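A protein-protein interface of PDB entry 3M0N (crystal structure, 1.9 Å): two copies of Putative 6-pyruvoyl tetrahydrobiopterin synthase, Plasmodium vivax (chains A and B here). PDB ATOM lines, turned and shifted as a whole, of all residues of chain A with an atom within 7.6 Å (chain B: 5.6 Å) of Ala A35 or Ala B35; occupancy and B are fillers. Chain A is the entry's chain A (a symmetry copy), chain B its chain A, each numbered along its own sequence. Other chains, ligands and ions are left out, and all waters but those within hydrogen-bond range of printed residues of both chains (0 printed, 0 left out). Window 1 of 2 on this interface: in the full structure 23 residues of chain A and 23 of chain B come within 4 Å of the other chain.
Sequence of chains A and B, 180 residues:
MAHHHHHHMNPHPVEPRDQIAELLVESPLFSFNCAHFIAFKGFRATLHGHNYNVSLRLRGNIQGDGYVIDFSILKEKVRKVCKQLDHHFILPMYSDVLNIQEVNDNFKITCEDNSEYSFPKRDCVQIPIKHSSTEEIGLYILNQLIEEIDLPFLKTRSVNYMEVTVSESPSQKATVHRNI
O of Leu A47 lies within hydrogen-bond range of N of Phe B89 (3.5 Å).
OD2 of Asp A123 lies within hydrogen-bond range of N of Leu B47 (2.8 Å).
The backbone carbonyl oxygen of Leu B47 lies close to the backbone carbonyl oxygen of His A87, 3.4 Å away.
The backbone carbonyl oxygen of Leu B47 lies close to the backbone NH of His A88 (3.5 Å).
N of His B88 sits close to O of Leu A47 (3.5 Å).
The backbone carbonyl oxygen (O) of Leu B47 is in hydrogen-bond range of the backbone NH (N) of Phe A89 (3.5 Å).
The backbone NH (N) of His A50 sits at hydrogen-bond distance from the backbone carbonyl oxygen (O) of Cys A34 (2.9 Å).
O of Asn A33 lies within hydrogen-bond range of N of His A87 (2.9 Å).
The backbone NH of Ala A35 is in hydrogen-bond range of the backbone carbonyl oxygen of His A88 (3.2 Å).
A ring nitrogen (ND1) of His A88 sits at hydrogen-bond distance from the backbone carbonyl oxygen of Asp A86 (2.8 Å).
N of Asn A33 lies within hydrogen-bond range of OD2 of Asp A86, 2.7 Å away.
The backbone carbonyl oxygen of Ala B35 is in hydrogen-bond range of the backbone NH of Ile B90 (3.0 Å).
O of Asn A33 touches CB of His B48, 3.1 Å away.
C of Cys A34 touches C of His B48, at 3.9 Å.
Ala A35 touches Ala B35 (CB to CB, 3.9 Å).
His B48 touches Ala A35 (O to CB, 3.6 Å).
His A48 touches Ala B35.
CA of Gly B49 touches CA of Gly A49, 3.9 Å away.
Gly A49 touches His B50.
O of His A50 touches O of Gly B49, at 3.5 Å.
CA of His A87 touches CB of His B48, at 3.5 Å.
CD1 of Phe A119 touches CD2 of Leu B47 (3.4 Å).
Printed residues of chain A within 4 Å of Ala B35: Ala A35 (3.9 Å), His A48 (3.6 Å) and Gly A49 (3.7 Å).
Of the printed residues of chain A, His B88 touches Leu A47 (3.3 Å).
Printed residues of chain A within 4 Å of Phe B89: Leu A47 (3.5 Å).
Tyr A52 touches none of the printed residues of chain B.
Val A125 touches none of the printed residues of chain B.
The nearest residue of chain B that does not touch Ala A35 is Leu B47 (4.05 Å).
The nearest printed residue of chain A that does not touch Phe B89 is His A48 (5.2 Å).
Of the 12 printed residues of chain B, 9 touch a printed residue of chain A.
Of the 22 printed residues of chain A, 12 touch a printed residue of chain B.
Hydrophobic or aromatic side chains of chain A that line the printed part of chain B: Ala A35, His A48, His A50, His A87 and Phe A119.
Along chain A the printed residues that touch a printed residue of chain B span positions 33 to 123.
Among the printed residues, no Asp or Glu carboxylate lies within 4 Å of a Lys or Arg side-chain nitrogen of the other chain.
Asn A33 touches His B50, and with the chains exchanged His A50 touches Asn B33.
Cys A34 touches His B48, and with the chains exchanged His A48 touches Cys B34.
Gly B49 touches its own counterpart, Gly A49.
His B50 touches its own counterpart, His A50.
Positions printed for both chains: 33, 34, 35, 36, 37, 47, 48, 49, 50, 88, 89 and 90.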
ATOM      1  N   PHE A  32      16.208   1.073   8.236  1.00  0.00           N
ATOM      2  CA  PHE A  32      17.040   1.641   7.193  1.00  0.00           C
ATOM      3  C   PHE A  32      17.747   0.507   6.485  1.00  0.00           C
ATOM      4  O   PHE A  32      18.455  -0.300   7.105  1.00  0.00           O
ATOM      5  CB  PHE A  32      18.002   2.721   7.698  1.00  0.00           C
ATOM      6  CG  PHE A  32      18.765   2.361   8.919  1.00  0.00           C
ATOM      7  CD1 PHE A  32      20.080   1.918   8.827  1.00  0.00           C
ATOM      8  CD2 PHE A  32      18.200   2.525  10.182  1.00  0.00           C
ATOM      9  CE1 PHE A  32      20.801   1.632   9.972  1.00  0.00           C
ATOM     10  CE2 PHE A  32      18.923   2.228  11.319  1.00  0.00           C
ATOM     11  CZ  PHE A  32      20.225   1.774  11.207  1.00  0.00           C
ATOM     12  N   ASN A  33      17.496   0.437   5.181  1.00  0.00           N
ATOM     13  CA  ASN A  33      18.007  -0.625   4.354  1.00  0.00           C
ATOM     14  C   ASN A  33      19.292  -0.106   3.701  1.00  0.00           C
ATOM     15  O   ASN A  33      19.243   0.701   2.764  1.00  0.00           O
ATOM     16  CB  ASN A  33      16.938  -1.017   3.335  1.00  0.00           C
ATOM     17  CG  ASN A  33      15.639  -1.512   4.002  1.00  0.00           C
ATOM     18  OD1 ASN A  33      15.574  -1.741   5.224  1.00  0.00           O
ATOM     19  ND2 ASN A  33      14.603  -1.679   3.197  1.00  0.00           N
ATOM     20  N   CYS A  34      20.433  -0.536   4.242  1.00  0.00           N
ATOM     21  CA  CYS A  34      21.722   0.034   3.914  1.00  0.00           C
ATOM     22  C   CYS A  34      22.755  -1.021   3.503  1.00  0.00           C
ATOM     23  O   CYS A  34      22.634  -2.192   3.875  1.00  0.00           O
ATOM     24  CB  CYS A  34      22.262   0.784   5.137  1.00  0.00           C
ATOM     25  SG  CYS A  34      21.355   2.328   5.477  1.00  0.00           S
ATOM     26  N   ALA A  35      23.760  -0.580   2.743  1.00  0.00           N
ATOM     27  CA  ALA A  35      24.936  -1.371   2.434  1.00  0.00           C
ATOM     28  C   ALA A  35      26.020  -0.960   3.415  1.00  0.00           C
ATOM     29  O   ALA A  35      26.030   0.182   3.888  1.00  0.00           O
ATOM     30  CB  ALA A  35      25.408  -1.121   0.994  1.00  0.00           C
ATOM     31  N   HIS A  36      26.945  -1.870   3.686  1.00  0.00           N
ATOM     32  CA  HIS A  36      28.110  -1.552   4.538  1.00  0.00           C
ATOM     33  C   HIS A  36      29.138  -2.664   4.373  1.00  0.00           C
ATOM     34  O   HIS A  36      28.899  -3.639   3.653  1.00  0.00           O
ATOM     35  CB  HIS A  36      27.698  -1.375   5.985  1.00  0.00           C
ATOM     36  CG  HIS A  36      27.686  -2.644   6.791  1.00  0.00           C
ATOM     37  ND1 HIS A  36      28.361  -2.760   7.989  1.00  0.00           N
ATOM     38  CD2 HIS A  36      27.062  -3.832   6.592  1.00  0.00           C
ATOM     39  CE1 HIS A  36      28.163  -3.971   8.488  1.00  0.00           C
ATOM     40  NE2 HIS A  36      27.376  -4.638   7.661  1.00  0.00           N
ATOM     41  N   PHE A  37      30.298  -2.494   4.970  1.00  0.00           N
ATOM     42  CA  PHE A  37      31.167  -3.615   5.178  1.00  0.00           C
ATOM     43  C   PHE A  37      31.960  -3.339   6.428  1.00  0.00           C
ATOM     44  O   PHE A  37      32.263  -2.199   6.723  1.00  0.00           O
ATOM     45  CB  PHE A  37      32.064  -3.952   3.951  1.00  0.00           C
ATOM     46  CG  PHE A  37      33.113  -2.890   3.570  1.00  0.00           C
ATOM     47  CD1 PHE A  37      34.347  -2.830   4.226  1.00  0.00           C
ATOM     48  CD2 PHE A  37      32.900  -2.037   2.481  1.00  0.00           C
ATOM     49  CE1 PHE A  37      35.332  -1.892   3.837  1.00  0.00           C
ATOM     50  CE2 PHE A  37      33.874  -1.110   2.078  1.00  0.00           C
ATOM     51  CZ  PHE A  37      35.086  -1.035   2.765  1.00  0.00           C
ATOM     52  N   LEU A  47      31.509  -6.395   0.680  1.00  0.00           N
ATOM     53  CA  LEU A  47      30.358  -5.507   0.626  1.00  0.00           C
ATOM     54  C   LEU A  47      29.052  -6.287   0.655  1.00  0.00           C
ATOM     55  O   LEU A  47      28.882  -7.272  -0.068  1.00  0.00           O
ATOM     56  CB  LEU A  47      30.404  -4.677  -0.646  1.00  0.00           C
ATOM     57  CG  LEU A  47      29.261  -3.675  -0.844  1.00  0.00           C
ATOM     58  CD1 LEU A  47      29.341  -2.587   0.227  1.00  0.00           C
ATOM     59  CD2 LEU A  47      29.360  -3.093  -2.246  1.00  0.00           C
ATOM     60  N   HIS A  48      28.130  -5.819   1.485  1.00  0.00           N
ATOM     61  CA  HIS A  48      26.832  -6.457   1.633  1.00  0.00           C
ATOM     62  C   HIS A  48      25.879  -5.433   2.227  1.00  0.00           C
ATOM     63  O   HIS A  48      26.151  -4.239   2.139  1.00  0.00           O
ATOM     64  CB  HIS A  48      26.951  -7.725   2.496  1.00  0.00           C
ATOM     65  CG  HIS A  48      27.375  -7.482   3.915  1.00  0.00           C
ATOM     66  ND1 HIS A  48      28.697  -7.354   4.289  1.00  0.00           N
ATOM     67  CD2 HIS A  48      26.652  -7.397   5.057  1.00  0.00           C
ATOM     68  CE1 HIS A  48      28.769  -7.176   5.596  1.00  0.00           C
ATOM     69  NE2 HIS A  48      27.542  -7.207   6.087  1.00  0.00           N
ATOM     70  N   GLY A  49      24.779  -5.884   2.818  1.00  0.00           N
ATOM     71  CA  GLY A  49      23.783  -4.975   3.348  1.00  0.00           C
ATOM     72  C   GLY A  49      22.813  -5.643   4.297  1.00  0.00           C
ATOM     73  O   GLY A  49      22.853  -6.864   4.489  1.00  0.00           O
ATOM     74  N   HIS A  50      21.951  -4.823   4.893  1.00  0.00           N
ATOM     75  CA  HIS A  50      20.984  -5.250   5.906  1.00  0.00           C
ATOM     76  C   HIS A  50      19.755  -4.354   5.923  1.00  0.00           C
ATOM     77  O   HIS A  50      19.829  -3.175   5.556  1.00  0.00           O
ATOM     78  CB  HIS A  50      21.570  -5.173   7.313  1.00  0.00           C
ATOM     79  CG  HIS A  50      22.818  -5.968   7.507  1.00  0.00           C
ATOM     80  ND1 HIS A  50      22.828  -7.347   7.553  1.00  0.00           N
ATOM     81  CD2 HIS A  50      24.096  -5.574   7.706  1.00  0.00           C
ATOM     82  CE1 HIS A  50      24.066  -7.767   7.750  1.00  0.00           C
ATOM     83  NE2 HIS A  50      24.852  -6.710   7.852  1.00  0.00           N
ATOM     84  N   TYR A  52      18.296  -2.827   8.638  1.00  0.00           N
ATOM     85  CA  TYR A  52      18.506  -2.523  10.047  1.00  0.00           C
ATOM     86  C   TYR A  52      17.174  -2.123  10.633  1.00  0.00           C
ATOM     87  O   TYR A  52      16.368  -1.487   9.957  1.00  0.00           O
ATOM     88  CB  TYR A  52      19.481  -1.366  10.220  1.00  0.00           C
ATOM     89  CG  TYR A  52      20.917  -1.665   9.858  1.00  0.00           C
ATOM     90  CD1 TYR A  52      21.831  -2.034  10.838  1.00  0.00           C
ATOM     91  CD2 TYR A  52      21.377  -1.519   8.551  1.00  0.00           C
ATOM     92  CE1 TYR A  52      23.154  -2.269  10.528  1.00  0.00           C
ATOM     93  CE2 TYR A  52      22.715  -1.757   8.230  1.00  0.00           C
ATOM     94  CZ  TYR A  52      23.594  -2.134   9.231  1.00  0.00           C
ATOM     95  OH  TYR A  52      24.918  -2.377   8.928  1.00  0.00           O
ATOM     96  N   LEU A  85      19.364   7.587   7.075  1.00  0.00           N
ATOM     97  CA  LEU A  85      20.311   6.516   6.823  1.00  0.00           C
ATOM     98  C   LEU A  85      19.845   5.601   5.676  1.00  0.00           C
ATOM     99  O   LEU A  85      20.657   5.126   4.887  1.00  0.00           O
ATOM    100  CB  LEU A  85      20.478   5.675   8.069  1.00  0.00           C
ATOM    101  CG  LEU A  85      21.096   6.342   9.298  1.00  0.00           C
ATOM    102  CD1 LEU A  85      21.046   5.393  10.485  1.00  0.00           C
ATOM    103  CD2 LEU A  85      22.501   6.719   8.996  1.00  0.00           C
ATOM    104  N   ASP A  86      18.542   5.382   5.602  1.00  0.00           N
ATOM    105  CA  ASP A  86      17.930   4.445   4.642  1.00  0.00           C
ATOM    106  C   ASP A  86      18.357   4.663   3.184  1.00  0.00           C
ATOM    107  O   ASP A  86      18.474   5.800   2.708  1.00  0.00           O
ATOM    108  CB  ASP A  86      16.409   4.547   4.770  1.00  0.00           C
ATOM    109  CG  ASP A  86      15.667   3.515   3.947  1.00  0.00           C
ATOM    110  OD1 ASP A  86      14.641   3.887   3.337  1.00  0.00           O
ATOM    111  OD2 ASP A  86      16.087   2.343   3.933  1.00  0.00           O
ATOM    112  N   HIS A  87      18.541   3.549   2.476  1.00  0.00           N
ATOM    113  CA  HIS A  87      18.947   3.522   1.066  1.00  0.00           C
ATOM    114  C   HIS A  87      20.313   4.187   0.764  1.00  0.00           C
ATOM    115  O   HIS A  87      20.480   4.844  -0.266  1.00  0.00           O
ATOM    116  CB  HIS A  87      17.807   4.052   0.171  1.00  0.00           C
ATOM    117  CG  HIS A  87      16.808   2.997  -0.194  1.00  0.00           C
ATOM    118  ND1 HIS A  87      16.379   2.791  -1.488  1.00  0.00           N
ATOM    119  CD2 HIS A  87      16.188   2.059   0.561  1.00  0.00           C
ATOM    120  CE1 HIS A  87      15.518   1.789  -1.510  1.00  0.00           C
ATOM    121  NE2 HIS A  87      15.385   1.326  -0.279  1.00  0.00           N
ATOM    122  N   HIS A  88      21.282   4.007   1.674  1.00  0.00           N
ATOM    123  CA  HIS A  88      22.638   4.520   1.511  1.00  0.00           C
ATOM    124  C   HIS A  88      23.668   3.488   1.942  1.00  0.00           C
ATOM    125  O   HIS A  88      23.349   2.543   2.687  1.00  0.00           O
ATOM    126  CB  HIS A  88      22.868   5.786   2.358  1.00  0.00           C
ATOM    127  CG  HIS A  88      22.107   6.974   1.865  1.00  0.00           C
ATOM    128  ND1 HIS A  88      20.824   7.257   2.279  1.00  0.00           N
ATOM    129  CD2 HIS A  88      22.440   7.941   0.980  1.00  0.00           C
ATOM    130  CE1 HIS A  88      20.401   8.351   1.672  1.00  0.00           C
ATOM    131  NE2 HIS A  88      21.361   8.787   0.878  1.00  0.00           N
ATOM    132  N   PHE A  89      24.895   3.680   1.456  1.00  0.00           N
ATOM    133  CA  PHE A  89      26.067   2.988   1.980  1.00  0.00           C
ATOM    134  C   PHE A  89      26.549   3.736   3.207  1.00  0.00           C
ATOM    135  O   PHE A  89      26.748   4.952   3.162  1.00  0.00           O
ATOM    136  CB  PHE A  89      27.184   2.898   0.932  1.00  0.00           C
ATOM    137  CG  PHE A  89      28.465   2.338   1.483  1.00  0.00           C
ATOM    138  CD1 PHE A  89      28.673   0.962   1.527  1.00  0.00           C
ATOM    139  CD2 PHE A  89      29.442   3.184   1.993  1.00  0.00           C
ATOM    140  CE1 PHE A  89      29.836   0.436   2.058  1.00  0.00           C
ATOM    141  CE2 PHE A  89      30.623   2.658   2.511  1.00  0.00           C
ATOM    142  CZ  PHE A  89      30.815   1.298   2.559  1.00  0.00           C
ATOM    143  N   ILE A  90      26.743   3.022   4.312  1.00  0.00           N
ATOM    144  CA  ILE A  90      27.100   3.658   5.568  1.00  0.00           C
ATOM    145  C   ILE A  90      28.593   3.741   5.647  1.00  0.00           C
ATOM    146  O   ILE A  90      29.275   2.722   5.652  1.00  0.00           O
ATOM    147  CB  ILE A  90      26.592   2.880   6.798  1.00  0.00           C
ATOM    148  CG1 ILE A  90      25.071   2.925   6.837  1.00  0.00           C
ATOM    149  CG2 ILE A  90      27.189   3.492   8.098  1.00  0.00           C
ATOM    150  CD1 ILE A  90      24.451   1.856   7.736  1.00  0.00           C
ATOM    151  N   LEU A  91      29.103   4.971   5.733  1.00  0.00           N
ATOM    152  CA  LEU A  91      30.519   5.213   5.623  1.00  0.00           C
ATOM    153  C   LEU A  91      31.033   5.795   6.917  1.00  0.00           C
ATOM    154  O   LEU A  91      30.675   6.921   7.275  1.00  0.00           O
ATOM    155  CB  LEU A  91      30.799   6.160   4.461  1.00  0.00           C
ATOM    156  CG  LEU A  91      32.249   6.447   4.081  1.00  0.00           C
ATOM    157  CD1 LEU A  91      33.008   5.163   3.802  1.00  0.00           C
ATOM    158  CD2 LEU A  91      32.301   7.379   2.882  1.00  0.00           C
ATOM    159  N   PHE A 119      32.125   4.777  -4.667  1.00  0.00           N
ATOM    160  CA  PHE A 119      30.669   5.064  -4.667  1.00  0.00           C
ATOM    161  C   PHE A 119      30.430   6.559  -4.892  1.00  0.00           C
ATOM    162  O   PHE A 119      31.206   7.401  -4.386  1.00  0.00           O
ATOM    163  CB  PHE A 119      29.990   4.720  -3.330  1.00  0.00           C
ATOM    164  CG  PHE A 119      30.396   3.392  -2.713  1.00  0.00           C
ATOM    165  CD1 PHE A 119      30.001   2.189  -3.264  1.00  0.00           C
ATOM    166  CD2 PHE A 119      31.135   3.356  -1.555  1.00  0.00           C
ATOM    167  CE1 PHE A 119      30.375   0.982  -2.651  1.00  0.00           C
ATOM    168  CE2 PHE A 119      31.482   2.155  -0.954  1.00  0.00           C
ATOM    169  CZ  PHE A 119      31.105   0.979  -1.502  1.00  0.00           C
ATOM    170  N   ASP A 123      25.379   8.559  -2.671  1.00  0.00           N
ATOM    171  CA  ASP A 123      24.940   7.210  -2.280  1.00  0.00           C
ATOM    172  C   ASP A 123      25.400   6.860  -0.858  1.00  0.00           C
ATOM    173  O   ASP A 123      24.992   5.838  -0.331  1.00  0.00           O
ATOM    174  CB  ASP A 123      25.473   6.113  -3.228  1.00  0.00           C
ATOM    175  CG  ASP A 123      24.722   6.036  -4.545  1.00  0.00           C
ATOM    176  OD1 ASP A 123      24.343   7.085  -5.090  1.00  0.00           O
ATOM    177  OD2 ASP A 123      24.512   4.901  -5.041  1.00  0.00           O
ATOM    178  N   VAL A 125      26.282   7.833   3.343  1.00  0.00           N
ATOM    179  CA  VAL A 125      26.012   8.668   4.501  1.00  0.00           C
ATOM    180  C   VAL A 125      27.240   8.579   5.373  1.00  0.00           C
ATOM    181  O   VAL A 125      27.664   7.495   5.781  1.00  0.00           O
ATOM    182  CB  VAL A 125      24.714   8.281   5.249  1.00  0.00           C
ATOM    183  CG1 VAL A 125      23.504   8.639   4.389  1.00  0.00           C
ATOM    184  CG2 VAL A 125      24.686   6.792   5.643  1.00  0.00           C
ATOM    185  N   SER A 132      31.235   0.486  11.070  1.00  0.00           N
ATOM    186  CA  SER A 132      29.810   0.348  10.826  1.00  0.00           C
ATOM    187  C   SER A 132      29.246  -0.901  11.541  1.00  0.00           C
ATOM    188  O   SER A 132      28.528  -1.710  10.936  1.00  0.00           O
ATOM    189  CB  SER A 132      29.510   0.334   9.307  1.00  0.00           C
ATOM    190  OG  SER A 132      30.248  -0.662   8.619  1.00  0.00           O
ATOM    191  N   ASN B  33      22.386 -11.689   3.019  1.00  0.00           N
ATOM    192  CA  ASN B  33      22.487 -10.296   3.365  1.00  0.00           C
ATOM    193  C   ASN B  33      23.372  -9.633   2.304  1.00  0.00           C
ATOM    194  O   ASN B  33      24.598  -9.801   2.312  1.00  0.00           O
ATOM    195  CB  ASN B  33      23.058 -10.175   4.777  1.00  0.00           C
ATOM    196  CG  ASN B  33      22.173 -10.867   5.833  1.00  0.00           C
ATOM    197  OD1 ASN B  33      21.034 -11.293   5.560  1.00  0.00           O
ATOM    198  ND2 ASN B  33      22.696 -10.979   7.042  1.00  0.00           N
ATOM    199  N   CYS B  34      22.732  -8.932   1.368  1.00  0.00           N
ATOM    200  CA  CYS B  34      23.380  -8.449   0.167  1.00  0.00           C
ATOM    201  C   CYS B  34      23.164  -6.950  -0.065  1.00  0.00           C
ATOM    202  O   CYS B  34      22.188  -6.374   0.427  1.00  0.00           O
ATOM    203  CB  CYS B  34      22.821  -9.208  -1.041  1.00  0.00           C
ATOM    204  SG  CYS B  34      23.379 -10.942  -1.105  1.00  0.00           S
ATOM    205  N   ALA B  35      24.081  -6.345  -0.823  1.00  0.00           N
ATOM    206  CA  ALA B  35      23.937  -4.992  -1.328  1.00  0.00           C
ATOM    207  C   ALA B  35      23.409  -5.100  -2.748  1.00  0.00           C
ATOM    208  O   ALA B  35      23.668  -6.096  -3.433  1.00  0.00           O
ATOM    209  CB  ALA B  35      25.282  -4.252  -1.323  1.00  0.00           C
ATOM    210  N   HIS B  36      22.708  -4.068  -3.196  1.00  0.00           N
ATOM    211  CA  HIS B  36      22.238  -4.009  -4.597  1.00  0.00           C
ATOM    212  C   HIS B  36      21.787  -2.583  -4.887  1.00  0.00           C
ATOM    213  O   HIS B  36      21.816  -1.722  -4.001  1.00  0.00           O
ATOM    214  CB  HIS B  36      21.130  -5.012  -4.844  1.00  0.00           C
ATOM    215  CG  HIS B  36      19.747  -4.503  -4.549  1.00  0.00           C
ATOM    216  ND1 HIS B  36      18.723  -4.575  -5.473  1.00  0.00           N
ATOM    217  CD2 HIS B  36      19.212  -3.945  -3.435  1.00  0.00           C
ATOM    218  CE1 HIS B  36      17.619  -4.073  -4.943  1.00  0.00           C
ATOM    219  NE2 HIS B  36      17.888  -3.688  -3.707  1.00  0.00           N
ATOM    220  N   PHE B  37      21.441  -2.310  -6.127  1.00  0.00           N
ATOM    221  CA  PHE B  37      20.671  -1.135  -6.412  1.00  0.00           C
ATOM    222  C   PHE B  37      19.832  -1.435  -7.627  1.00  0.00           C
ATOM    223  O   PHE B  37      20.248  -2.184  -8.490  1.00  0.00           O
ATOM    224  CB  PHE B  37      21.527   0.156  -6.569  1.00  0.00           C
ATOM    225  CG  PHE B  37      22.487   0.186  -7.774  1.00  0.00           C
ATOM    226  CD1 PHE B  37      22.034   0.551  -9.046  1.00  0.00           C
ATOM    227  CD2 PHE B  37      23.857  -0.036  -7.599  1.00  0.00           C
ATOM    228  CE1 PHE B  37      22.927   0.635 -10.140  1.00  0.00           C
ATOM    229  CE2 PHE B  37      24.756   0.055  -8.672  1.00  0.00           C
ATOM    230  CZ  PHE B  37      24.284   0.382  -9.945  1.00  0.00           C
ATOM    231  N   LEU B  47      22.809   2.994  -3.872  1.00  0.00           N
ATOM    232  CA  LEU B  47      23.308   1.751  -3.304  1.00  0.00           C
ATOM    233  C   LEU B  47      22.787   1.538  -1.890  1.00  0.00           C
ATOM    234  O   LEU B  47      22.816   2.446  -1.056  1.00  0.00           O
ATOM    235  CB  LEU B  47      24.828   1.773  -3.267  1.00  0.00           C
ATOM    236  CG  LEU B  47      25.510   0.520  -2.706  1.00  0.00           C
ATOM    237  CD1 LEU B  47      25.250  -0.666  -3.634  1.00  0.00           C
ATOM    238  CD2 LEU B  47      26.997   0.801  -2.556  1.00  0.00           C
ATOM    239  N   HIS B  48      22.331   0.320  -1.632  1.00  0.00           N
ATOM    240  CA  HIS B  48      21.792  -0.041  -0.331  1.00  0.00           C
ATOM    241  C   HIS B  48      21.844  -1.555  -0.214  1.00  0.00           C
ATOM    242  O   HIS B  48      22.605  -2.187  -0.941  1.00  0.00           O
ATOM    243  CB  HIS B  48      20.369   0.517  -0.165  1.00  0.00           C
ATOM    244  CG  HIS B  48      19.356  -0.046  -1.120  1.00  0.00           C
ATOM    245  ND1 HIS B  48      19.177   0.449  -2.396  1.00  0.00           N
ATOM    246  CD2 HIS B  48      18.435  -1.025  -0.964  1.00  0.00           C
ATOM    247  CE1 HIS B  48      18.207  -0.219  -2.993  1.00  0.00           C
ATOM    248  NE2 HIS B  48      17.733  -1.112  -2.142  1.00  0.00           N
ATOM    249  N   GLY B  49      21.055  -2.132   0.685  1.00  0.00           N
ATOM    250  CA  GLY B  49      21.092  -3.562   0.912  1.00  0.00           C
ATOM    251  C   GLY B  49      19.892  -4.075   1.675  1.00  0.00           C
ATOM    252  O   GLY B  49      19.044  -3.293   2.122  1.00  0.00           O
ATOM    253  N   HIS B  50      19.830  -5.398   1.809  1.00  0.00           N
ATOM    254  CA  HIS B  50      18.714  -6.104   2.440  1.00  0.00           C
ATOM    255  C   HIS B  50      19.155  -7.428   3.045  1.00  0.00           C
ATOM    256  O   HIS B  50      20.129  -8.037   2.584  1.00  0.00           O
ATOM    257  CB  HIS B  50      17.625  -6.454   1.430  1.00  0.00           C
ATOM    258  CG  HIS B  50      17.067  -5.283   0.692  1.00  0.00           C
ATOM    259  ND1 HIS B  50      16.248  -4.344   1.284  1.00  0.00           N
ATOM    260  CD2 HIS B  50      17.181  -4.921  -0.606  1.00  0.00           C
ATOM    261  CE1 HIS B  50      15.900  -3.441   0.384  1.00  0.00           C
ATOM    262  NE2 HIS B  50      16.448  -3.772  -0.771  1.00  0.00           N
ATOM    263  N   HIS B  88      27.456 -10.443  -0.462  1.00  0.00           N
ATOM    264  CA  HIS B  88      27.939  -9.957  -1.750  1.00  0.00           C
ATOM    265  C   HIS B  88      27.043  -8.850  -2.287  1.00  0.00           C
ATOM    266  O   HIS B  88      25.880  -8.712  -1.862  1.00  0.00           O
ATOM    267  CB  HIS B  88      27.969 -11.081  -2.803  1.00  0.00           C
ATOM    268  CG  HIS B  88      29.015 -12.113  -2.536  1.00  0.00           C
ATOM    269  ND1 HIS B  88      28.782 -13.221  -1.752  1.00  0.00           N
ATOM    270  CD2 HIS B  88      30.306 -12.197  -2.932  1.00  0.00           C
ATOM    271  CE1 HIS B  88      29.883 -13.946  -1.680  1.00  0.00           C
ATOM    272  NE2 HIS B  88      30.824 -13.348  -2.387  1.00  0.00           N
ATOM    273  N   PHE B  89      27.603  -8.071  -3.212  1.00  0.00           N
ATOM    274  CA  PHE B  89      26.830  -7.162  -4.050  1.00  0.00           C
ATOM    275  C   PHE B  89      26.265  -7.955  -5.212  1.00  0.00           C
ATOM    276  O   PHE B  89      27.000  -8.663  -5.904  1.00  0.00           O
ATOM    277  CB  PHE B  89      27.688  -5.998  -4.560  1.00  0.00           C
ATOM    278  CG  PHE B  89      26.971  -5.131  -5.557  1.00  0.00           C
ATOM    279  CD1 PHE B  89      26.164  -4.081  -5.129  1.00  0.00           C
ATOM    280  CD2 PHE B  89      27.073  -5.389  -6.919  1.00  0.00           C
ATOM    281  CE1 PHE B  89      25.478  -3.295  -6.036  1.00  0.00           C
ATOM    282  CE2 PHE B  89      26.399  -4.588  -7.837  1.00  0.00           C
ATOM    283  CZ  PHE B  89      25.596  -3.560  -7.403  1.00  0.00           C
ATOM    284  N   ILE B  90      24.958  -7.846  -5.439  1.00  0.00           N
ATOM    285  CA  ILE B  90      24.301  -8.645  -6.458  1.00  0.00           C
ATOM    286  C   ILE B  90      24.347  -7.892  -7.751  1.00  0.00           C
ATOM    287  O   ILE B  90      23.794  -6.802  -7.858  1.00  0.00           O
ATOM    288  CB  ILE B  90      22.827  -8.946  -6.123  1.00  0.00           C
ATOM    289  CG1 ILE B  90      22.755  -9.857  -4.906  1.00  0.00           C
ATOM    290  CG2 ILE B  90      22.130  -9.612  -7.345  1.00  0.00           C
ATOM    291  CD1 ILE B  90      21.384  -9.872  -4.233  1.00  0.00           C
